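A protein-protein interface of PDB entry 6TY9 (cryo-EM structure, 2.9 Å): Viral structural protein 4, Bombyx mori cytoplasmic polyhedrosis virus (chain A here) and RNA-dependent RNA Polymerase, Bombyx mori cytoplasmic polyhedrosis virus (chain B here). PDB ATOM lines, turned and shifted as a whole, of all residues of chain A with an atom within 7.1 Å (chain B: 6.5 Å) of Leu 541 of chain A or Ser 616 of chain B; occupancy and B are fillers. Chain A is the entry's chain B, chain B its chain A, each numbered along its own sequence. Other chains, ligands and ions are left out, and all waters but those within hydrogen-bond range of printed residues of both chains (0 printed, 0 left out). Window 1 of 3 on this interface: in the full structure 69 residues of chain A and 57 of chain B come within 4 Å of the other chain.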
ATOM      1  N   ASN A 492      -6.455   3.744   1.799  1.00  0.00           N
ATOM      2  CA  ASN A 492      -5.834   2.585   2.424  1.00  0.00           C
ATOM      3  C   ASN A 492      -5.690   2.714   3.932  1.00  0.00           C
ATOM      4  O   ASN A 492      -5.509   1.694   4.601  1.00  0.00           O
ATOM      5  CB  ASN A 492      -4.458   2.332   1.815  1.00  0.00           C
ATOM      6  CG  ASN A 492      -4.534   1.790   0.411  1.00  0.00           C
ATOM      7  OD1 ASN A 492      -3.656   2.038  -0.410  1.00  0.00           O
ATOM      8  ND2 ASN A 492      -5.587   1.039   0.126  1.00  0.00           N
ATOM      9  N   THR A 504      -9.337  -7.769   0.983  1.00  0.00           N
ATOM     10  CA  THR A 504      -9.595  -6.415   0.521  1.00  0.00           C
ATOM     11  C   THR A 504      -9.127  -6.295  -0.920  1.00  0.00           C
ATOM     12  O   THR A 504      -8.034  -6.750  -1.266  1.00  0.00           O
ATOM     13  CB  THR A 504      -8.894  -5.359   1.388  1.00  0.00           C
ATOM     14  OG1 THR A 504      -7.481  -5.456   1.214  1.00  0.00           O
ATOM     15  CG2 THR A 504      -9.215  -5.563   2.849  1.00  0.00           C
ATOM     16  N   LEU A 506      -9.326  -3.759  -4.747  1.00  0.00           N
ATOM     17  CA  LEU A 506      -9.460  -2.422  -5.316  1.00  0.00           C
ATOM     18  C   LEU A 506     -10.211  -2.569  -6.634  1.00  0.00           C
ATOM     19  O   LEU A 506      -9.798  -3.337  -7.506  1.00  0.00           O
ATOM     20  CB  LEU A 506      -8.104  -1.759  -5.511  1.00  0.00           C
ATOM     21  CG  LEU A 506      -8.119  -0.283  -5.902  1.00  0.00           C
ATOM     22  CD1 LEU A 506      -7.044   0.464  -5.169  1.00  0.00           C
ATOM     23  CD2 LEU A 506      -7.901  -0.148  -7.379  1.00  0.00           C
ATOM     24  N   LEU A 538      -4.647   6.552  -1.837  1.00  0.00           N
ATOM     25  CA  LEU A 538      -5.065   5.224  -2.283  1.00  0.00           C
ATOM     26  C   LEU A 538      -4.205   4.770  -3.456  1.00  0.00           C
ATOM     27  O   LEU A 538      -4.603   4.923  -4.620  1.00  0.00           O
ATOM     28  CB  LEU A 538      -6.543   5.223  -2.663  1.00  0.00           C
ATOM     29  CG  LEU A 538      -7.170   3.915  -3.145  1.00  0.00           C
ATOM     30  CD1 LEU A 538      -7.375   2.971  -1.995  1.00  0.00           C
ATOM     31  CD2 LEU A 538      -8.481   4.177  -3.848  1.00  0.00           C
ATOM     32  N   PRO A 539      -3.029   4.222  -3.197  1.00  0.00           N
ATOM     33  CA  PRO A 539      -2.279   3.522  -4.240  1.00  0.00           C
ATOM     34  C   PRO A 539      -2.927   2.176  -4.541  1.00  0.00           C
ATOM     35  O   PRO A 539      -3.847   1.731  -3.860  1.00  0.00           O
ATOM     36  CB  PRO A 539      -0.892   3.342  -3.625  1.00  0.00           C
ATOM     37  CG  PRO A 539      -0.839   4.268  -2.495  1.00  0.00           C
ATOM     38  CD  PRO A 539      -2.221   4.407  -1.986  1.00  0.00           C
ATOM     39  N   ALA A 540      -2.423   1.523  -5.581  1.00  0.00           N
ATOM     40  CA  ALA A 540      -2.912   0.204  -5.966  1.00  0.00           C
ATOM     41  C   ALA A 540      -2.040  -0.867  -5.319  1.00  0.00           C
ATOM     42  O   ALA A 540      -1.307  -1.604  -5.972  1.00  0.00           O
ATOM     43  CB  ALA A 540      -2.939   0.070  -7.483  1.00  0.00           C
ATOM     44  N   LEU A 541      -2.133  -0.928  -3.994  1.00  0.00           N
ATOM     45  CA  LEU A 541      -1.362  -1.865  -3.197  1.00  0.00           C
ATOM     46  C   LEU A 541      -2.164  -3.093  -2.796  1.00  0.00           C
ATOM     47  O   LEU A 541      -1.599  -4.024  -2.220  1.00  0.00           O
ATOM     48  CB  LEU A 541      -0.817  -1.165  -1.957  1.00  0.00           C
ATOM     49  CG  LEU A 541       0.110   0.003  -2.272  1.00  0.00           C
ATOM     50  CD1 LEU A 541       0.484   0.720  -1.004  1.00  0.00           C
ATOM     51  CD2 LEU A 541       1.341  -0.480  -2.993  1.00  0.00           C
ATOM     52  N   HIS A 542      -3.456  -3.118  -3.085  1.00  0.00           N
ATOM     53  CA  HIS A 542      -4.302  -4.286  -2.904  1.00  0.00           C
ATOM     54  C   HIS A 542      -4.697  -4.825  -4.273  1.00  0.00           C
ATOM     55  O   HIS A 542      -4.585  -4.136  -5.287  1.00  0.00           O
ATOM     56  CB  HIS A 542      -5.531  -3.942  -2.063  1.00  0.00           C
ATOM     57  CG  HIS A 542      -5.225  -3.727  -0.615  1.00  0.00           C
ATOM     58  ND1 HIS A 542      -5.417  -2.519   0.014  1.00  0.00           N
ATOM     59  CD2 HIS A 542      -4.731  -4.566   0.323  1.00  0.00           C
ATOM     60  CE1 HIS A 542      -5.058  -2.623   1.281  1.00  0.00           C
ATOM     61  NE2 HIS A 542      -4.635  -3.854   1.493  1.00  0.00           N
ATOM     62  N   THR A 543      -5.163  -6.069  -4.296  1.00  0.00           N
ATOM     63  CA  THR A 543      -5.431  -6.753  -5.553  1.00  0.00           C
ATOM     64  C   THR A 543      -6.509  -6.028  -6.346  1.00  0.00           C
ATOM     65  O   THR A 543      -7.548  -5.652  -5.802  1.00  0.00           O
ATOM     66  CB  THR A 543      -5.846  -8.196  -5.286  1.00  0.00           C
ATOM     67  OG1 THR A 543      -4.785  -8.875  -4.608  1.00  0.00           O
ATOM     68  CG2 THR A 543      -6.133  -8.916  -6.576  1.00  0.00           C
ATOM     69  N   THR A 544      -6.255  -5.834  -7.637  1.00  0.00           N
ATOM     70  CA  THR A 544      -7.174  -5.116  -8.506  1.00  0.00           C
ATOM     71  C   THR A 544      -8.146  -6.089  -9.154  1.00  0.00           C
ATOM     72  O   THR A 544      -7.744  -7.148  -9.642  1.00  0.00           O
ATOM     73  CB  THR A 544      -6.399  -4.349  -9.575  1.00  0.00           C
ATOM     74  OG1 THR A 544      -5.756  -3.220  -8.978  1.00  0.00           O
ATOM     75  CG2 THR A 544      -7.320  -3.860 -10.670  1.00  0.00           C
ATOM     76  N   GLN B 383       8.003   4.324  -9.566  1.00  0.00           N
ATOM     77  CA  GLN B 383       7.344   5.455  -8.937  1.00  0.00           C
ATOM     78  C   GLN B 383       8.390   6.381  -8.343  1.00  0.00           C
ATOM     79  O   GLN B 383       9.573   6.046  -8.271  1.00  0.00           O
ATOM     80  CB  GLN B 383       6.358   4.997  -7.865  1.00  0.00           C
ATOM     81  CG  GLN B 383       6.976   4.136  -6.806  1.00  0.00           C
ATOM     82  CD  GLN B 383       5.995   3.157  -6.229  1.00  0.00           C
ATOM     83  OE1 GLN B 383       4.914   2.957  -6.772  1.00  0.00           O
ATOM     84  NE2 GLN B 383       6.360   2.540  -5.119  1.00  0.00           N
ATOM     85  N   ARG B 496       3.975 -17.698  -0.229  1.00  0.00           N
ATOM     86  CA  ARG B 496       3.944 -16.306   0.184  1.00  0.00           C
ATOM     87  C   ARG B 496       5.274 -15.864   0.773  1.00  0.00           C
ATOM     88  O   ARG B 496       5.638 -14.691   0.653  1.00  0.00           O
ATOM     89  CB  ARG B 496       2.814 -16.080   1.183  1.00  0.00           C
ATOM     90  CG  ARG B 496       2.147 -14.733   1.035  1.00  0.00           C
ATOM     91  CD  ARG B 496       1.258 -14.439   2.211  1.00  0.00           C
ATOM     92  NE  ARG B 496      -0.107 -14.883   1.975  1.00  0.00           N
ATOM     93  CZ  ARG B 496      -1.065 -14.103   1.495  1.00  0.00           C
ATOM     94  NH1 ARG B 496      -0.803 -12.837   1.200  1.00  0.00           N
ATOM     95  NH2 ARG B 496      -2.281 -14.588   1.311  1.00  0.00           N
ATOM     96  N   THR B 557      -0.287   0.638   5.197  1.00  0.00           N
ATOM     97  CA  THR B 557      -0.156   0.180   3.820  1.00  0.00           C
ATOM     98  C   THR B 557       0.628   1.173   2.972  1.00  0.00           C
ATOM     99  O   THR B 557       1.395   0.770   2.093  1.00  0.00           O
ATOM    100  CB  THR B 557      -1.540  -0.066   3.223  1.00  0.00           C
ATOM    101  OG1 THR B 557      -2.266  -0.963   4.067  1.00  0.00           O
ATOM    102  CG2 THR B 557      -1.428  -0.676   1.848  1.00  0.00           C
ATOM    103  N   ASN B 558       0.457   2.473   3.221  1.00  0.00           N
ATOM    104  CA  ASN B 558       1.175   3.469   2.436  1.00  0.00           C
ATOM    105  C   ASN B 558       2.586   3.695   2.955  1.00  0.00           C
ATOM    106  O   ASN B 558       3.447   4.166   2.208  1.00  0.00           O
ATOM    107  CB  ASN B 558       0.411   4.787   2.419  1.00  0.00           C
ATOM    108  CG  ASN B 558      -0.858   4.714   1.608  1.00  0.00           C
ATOM    109  OD1 ASN B 558      -1.191   3.674   1.049  1.00  0.00           O
ATOM    110  ND2 ASN B 558      -1.571   5.822   1.535  1.00  0.00           N
ATOM    111  N   THR B 559       2.847   3.389   4.224  1.00  0.00           N
ATOM    112  CA  THR B 559       4.216   3.466   4.716  1.00  0.00           C
ATOM    113  C   THR B 559       5.088   2.391   4.087  1.00  0.00           C
ATOM    114  O   THR B 559       6.283   2.610   3.863  1.00  0.00           O
ATOM    115  CB  THR B 559       4.243   3.341   6.238  1.00  0.00           C
ATOM    116  OG1 THR B 559       3.330   4.280   6.811  1.00  0.00           O
ATOM    117  CG2 THR B 559       5.630   3.618   6.768  1.00  0.00           C
ATOM    118  N   LYS B 560       4.510   1.227   3.794  1.00  0.00           N
ATOM    119  CA  LYS B 560       5.267   0.154   3.162  1.00  0.00           C
ATOM    120  C   LYS B 560       5.715   0.546   1.762  1.00  0.00           C
ATOM    121  O   LYS B 560       6.689  -0.005   1.241  1.00  0.00           O
ATOM    122  CB  LYS B 560       4.412  -1.114   3.150  1.00  0.00           C
ATOM    123  CG  LYS B 560       4.858  -2.212   2.216  1.00  0.00           C
ATOM    124  CD  LYS B 560       5.930  -3.058   2.837  1.00  0.00           C
ATOM    125  CE  LYS B 560       6.493  -4.041   1.835  1.00  0.00           C
ATOM    126  NZ  LYS B 560       5.416  -4.626   0.997  1.00  0.00           N
ATOM    127  N   ASP B 561       5.042   1.522   1.156  1.00  0.00           N
ATOM    128  CA  ASP B 561       5.374   1.974  -0.186  1.00  0.00           C
ATOM    129  C   ASP B 561       6.707   2.704  -0.252  1.00  0.00           C
ATOM    130  O   ASP B 561       7.287   2.798  -1.335  1.00  0.00           O
ATOM    131  CB  ASP B 561       4.261   2.883  -0.701  1.00  0.00           C
ATOM    132  CG  ASP B 561       4.032   2.745  -2.186  1.00  0.00           C
ATOM    133  OD1 ASP B 561       4.773   1.985  -2.839  1.00  0.00           O
ATOM    134  OD2 ASP B 561       3.106   3.398  -2.703  1.00  0.00           O
ATOM    135  N   ASN B 564       8.948   0.001  -1.003  1.00  0.00           N
ATOM    136  CA  ASN B 564       8.670  -0.486  -2.348  1.00  0.00           C
ATOM    137  C   ASN B 564       9.353   0.375  -3.395  1.00  0.00           C
ATOM    138  O   ASN B 564       9.869  -0.141  -4.390  1.00  0.00           O
ATOM    139  CB  ASN B 564       7.164  -0.513  -2.600  1.00  0.00           C
ATOM    140  CG  ASN B 564       6.449  -1.554  -1.774  1.00  0.00           C
ATOM    141  OD1 ASN B 564       7.049  -2.515  -1.309  1.00  0.00           O
ATOM    142  ND2 ASN B 564       5.153  -1.368  -1.595  1.00  0.00           N
ATOM    143  N   LEU B 611       4.766  -7.725  -8.658  1.00  0.00           N
ATOM    144  CA  LEU B 611       3.579  -8.482  -8.287  1.00  0.00           C
ATOM    145  C   LEU B 611       3.387  -8.515  -6.779  1.00  0.00           C
ATOM    146  O   LEU B 611       2.255  -8.422  -6.300  1.00  0.00           O
ATOM    147  CB  LEU B 611       3.674  -9.901  -8.845  1.00  0.00           C
ATOM    148  CG  LEU B 611       2.401 -10.743  -8.879  1.00  0.00           C
ATOM    149  CD1 LEU B 611       2.388 -11.584 -10.128  1.00  0.00           C
ATOM    150  CD2 LEU B 611       2.291 -11.628  -7.657  1.00  0.00           C
ATOM    151  N   GLU B 612       4.476  -8.643  -6.023  1.00  0.00           N
ATOM    152  CA  GLU B 612       4.370  -8.696  -4.571  1.00  0.00           C
ATOM    153  C   GLU B 612       3.891  -7.371  -3.996  1.00  0.00           C
ATOM    154  O   GLU B 612       3.091  -7.349  -3.057  1.00  0.00           O
ATOM    155  CB  GLU B 612       5.720  -9.084  -3.970  1.00  0.00           C
ATOM    156  CG  GLU B 612       5.702  -9.287  -2.473  1.00  0.00           C
ATOM    157  CD  GLU B 612       6.169  -8.067  -1.714  1.00  0.00           C
ATOM    158  OE1 GLU B 612       6.644  -7.115  -2.361  1.00  0.00           O
ATOM    159  OE2 GLU B 612       6.063  -8.060  -0.470  1.00  0.00           O
ATOM    160  N   ALA B 613       4.370  -6.256  -4.545  1.00  0.00           N
ATOM    161  CA  ALA B 613       4.036  -4.952  -3.987  1.00  0.00           C
ATOM    162  C   ALA B 613       2.599  -4.550  -4.281  1.00  0.00           C
ATOM    163  O   ALA B 613       2.073  -3.640  -3.635  1.00  0.00           O
ATOM    164  CB  ALA B 613       4.995  -3.894  -4.524  1.00  0.00           C
ATOM    165  N   ALA B 614       1.950  -5.201  -5.240  1.00  0.00           N
ATOM    166  CA  ALA B 614       0.594  -4.822  -5.608  1.00  0.00           C
ATOM    167  C   ALA B 614      -0.453  -5.815  -5.138  1.00  0.00           C
ATOM    168  O   ALA B 614      -1.643  -5.575  -5.349  1.00  0.00           O
ATOM    169  CB  ALA B 614       0.485  -4.648  -7.121  1.00  0.00           C
ATOM    170  N   ASN B 615      -0.048  -6.920  -4.522  1.00  0.00           N
ATOM    171  CA  ASN B 615      -0.968  -7.895  -3.938  1.00  0.00           C
ATOM    172  C   ASN B 615      -0.534  -8.076  -2.494  1.00  0.00           C
ATOM    173  O   ASN B 615       0.183  -9.020  -2.164  1.00  0.00           O
ATOM    174  CB  ASN B 615      -0.935  -9.201  -4.698  1.00  0.00           C
ATOM    175  CG  ASN B 615      -1.261  -9.031  -6.151  1.00  0.00           C
ATOM    176  OD1 ASN B 615      -2.348  -8.593  -6.507  1.00  0.00           O
ATOM    177  ND2 ASN B 615      -0.315  -9.372  -7.008  1.00  0.00           N
ATOM    178  N   SER B 616      -0.908  -7.110  -1.673  1.00  0.00           N
ATOM    179  CA  SER B 616      -0.535  -7.183  -0.291  1.00  0.00           C
ATOM    180  C   SER B 616      -1.721  -7.350   0.628  1.00  0.00           C
ATOM    181  O   SER B 616      -2.576  -6.476   0.755  1.00  0.00           O
ATOM    182  CB  SER B 616       0.258  -5.937   0.107  1.00  0.00           C
ATOM    183  OG  SER B 616       0.785  -6.067   1.416  1.00  0.00           O
ATOM    184  N   GLN B 617      -1.745  -8.506   1.263  1.00  0.00           N
ATOM    185  CA  GLN B 617      -2.712  -8.821   2.300  1.00  0.00           C
ATOM    186  C   GLN B 617      -1.922  -9.197   3.544  1.00  0.00           C
ATOM    187  O   GLN B 617      -1.296 -10.259   3.582  1.00  0.00           O
ATOM    188  CB  GLN B 617      -3.618  -9.966   1.863  1.00  0.00           C
ATOM    189  CG  GLN B 617      -4.895 -10.100   2.648  1.00  0.00           C
ATOM    190  CD  GLN B 617      -5.872  -8.989   2.339  1.00  0.00           C
ATOM    191  OE1 GLN B 617      -6.107  -8.105   3.153  1.00  0.00           O
ATOM    192  NE2 GLN B 617      -6.444  -9.029   1.142  1.00  0.00           N
ATOM    193  N   THR B 618      -1.933  -8.326   4.547  1.00  0.00           N
ATOM    194  CA  THR B 618      -1.147  -8.549   5.747  1.00  0.00           C
ATOM    195  C   THR B 618      -1.942  -9.129   6.904  1.00  0.00           C
ATOM    196  O   THR B 618      -1.351  -9.423   7.948  1.00  0.00           O
ATOM    197  CB  THR B 618      -0.482  -7.242   6.207  1.00  0.00           C
ATOM    198  OG1 THR B 618      -1.398  -6.153   6.054  1.00  0.00           O
ATOM    199  CG2 THR B 618       0.757  -6.965   5.396  1.00  0.00           C
ATOM    200  N   GLU B 634      -6.386  -5.003   8.739  1.00  0.00           N
ATOM    201  CA  GLU B 634      -5.320  -4.916   7.751  1.00  0.00           C
ATOM    202  C   GLU B 634      -4.352  -3.776   8.045  1.00  0.00           C
ATOM    203  O   GLU B 634      -4.755  -2.697   8.485  1.00  0.00           O
ATOM    204  CB  GLU B 634      -5.918  -4.739   6.358  1.00  0.00           C
ATOM    205  CG  GLU B 634      -4.904  -4.772   5.250  1.00  0.00           C
ATOM    206  CD  GLU B 634      -4.522  -6.172   4.873  1.00  0.00           C
ATOM    207  OE1 GLU B 634      -3.585  -6.334   4.069  1.00  0.00           O
ATOM    208  OE2 GLU B 634      -5.151  -7.112   5.398  1.00  0.00           O
ATOM    209  N   ARG B 641       8.554 -13.091   7.882  1.00  0.00           N
ATOM    210  CA  ARG B 641       8.859 -12.838   6.481  1.00  0.00           C
ATOM    211  C   ARG B 641      10.370 -12.848   6.348  1.00  0.00           C
ATOM    212  O   ARG B 641      11.095 -12.884   7.345  1.00  0.00           O
ATOM    213  CB  ARG B 641       8.301 -11.498   5.985  1.00  0.00           C
ATOM    214  CG  ARG B 641       6.842 -11.522   5.590  1.00  0.00           C
ATOM    215  CD  ARG B 641       6.361 -10.193   5.068  1.00  0.00           C
ATOM    216  NE  ARG B 641       6.851  -9.921   3.727  1.00  0.00           N
ATOM    217  CZ  ARG B 641       6.543  -8.833   3.034  1.00  0.00           C
ATOM    218  NH1 ARG B 641       7.029  -8.657   1.816  1.00  0.00           N
ATOM    219  NH2 ARG B 641       5.738  -7.926   3.561  1.00  0.00           N
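Of the printed residues of chain B, Asn 492 of chain A touches Asn 558. Of the printed residues of chain B, Leu 541 of chain A touches Thr 557 (3.2 Å), Asn 558 (3.97 Å), Ala 613 (3.3 Å), Ala 614 (3.5 Å) and Ser 616 (3.2 Å). Of the printed residues of chain A, Ala 613 of chain B touches Leu 541. Printed residues of chain A within 4 Å of Asn 615 of chain B: Thr 543. Ser 616 of chain B touches just these residues of chain A: Leu 541 and His 542.
The backbone carbonyl oxygen of Leu 611 of chain B is in hydrogen-bond range of the side-chain amide nitrogen of Asn 615 of chain B (2.8 Å). The side-chain amide oxygen (OE1) of Gln 617 of chain B lies close to the side-chain carboxylate (OE2) of Glu 634 of chain B (2.6 Å). N of Thr 618 of chain B lies within hydrogen-bond range of OE1 of Glu 634 of chain B, 2.6 Å away. The side-chain amide oxygen (OD1) of Asn 492 of chain A lies close to the backbone carbonyl oxygen (O) of Pro 539 of chain A (3.5 Å). OG1 of Thr 504 of chain A sits close to NE2 of His 542 of chain A (3.3 Å). O of Thr 543 of chain A lies within hydrogen-bond range of N of Leu 506 of chain A (2.8 Å).
OD1 of Asn 558 of chain B lies close to OD1 of Asn 492 of chain A (3.3 Å). OD1 of Asn 615 of chain B is in hydrogen-bond range of OG1 of Thr 543 of chain A. The backbone carbonyl oxygen (O) of Leu 541 of chain A sits at hydrogen-bond distance from the backbone NH (N) of Ser 616 of chain B. O of Ser 616 of chain B sits close to NE2 of His 542 of chain A, 3.4 Å away. N of Thr 504 of chain A sits close to NE2 of Gln 617 of chain B (3.2 Å). The backbone carbonyl oxygen of Leu 541 of chain A lies close to the backbone carbonyl oxygen of Ala 614 of chain B (3.5 Å). O of His 542 of chain A sits close to O of Ala 614 of chain B (3.3 Å).
Among the printed residues, merely in contact across the chains: Leu 541 of chain A with Thr 557 of chain B (3.2 Å), Pro 539 of chain A with Asn 558 of chain B (3.3 Å), Leu 541 of chain A with Ala 613 of chain B (3.3 Å), Thr 543 of chain A with Ala 614 of chain B (3.7 Å), Ala 540 of chain A with Ala 614 of chain B (3.7 Å), His 542 of chain A with Glu 634 of chain B (3.7 Å) and Leu 541 of chain A with Asn 558 of chain B (3.97 Å).
Of the 10 printed residues of chain A, 7 touch a printed residue of chain B. Of the 18 printed residues of chain B, 8 touch a printed residue of chain A. Among the printed residues, 14 pairs touch across the chains.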
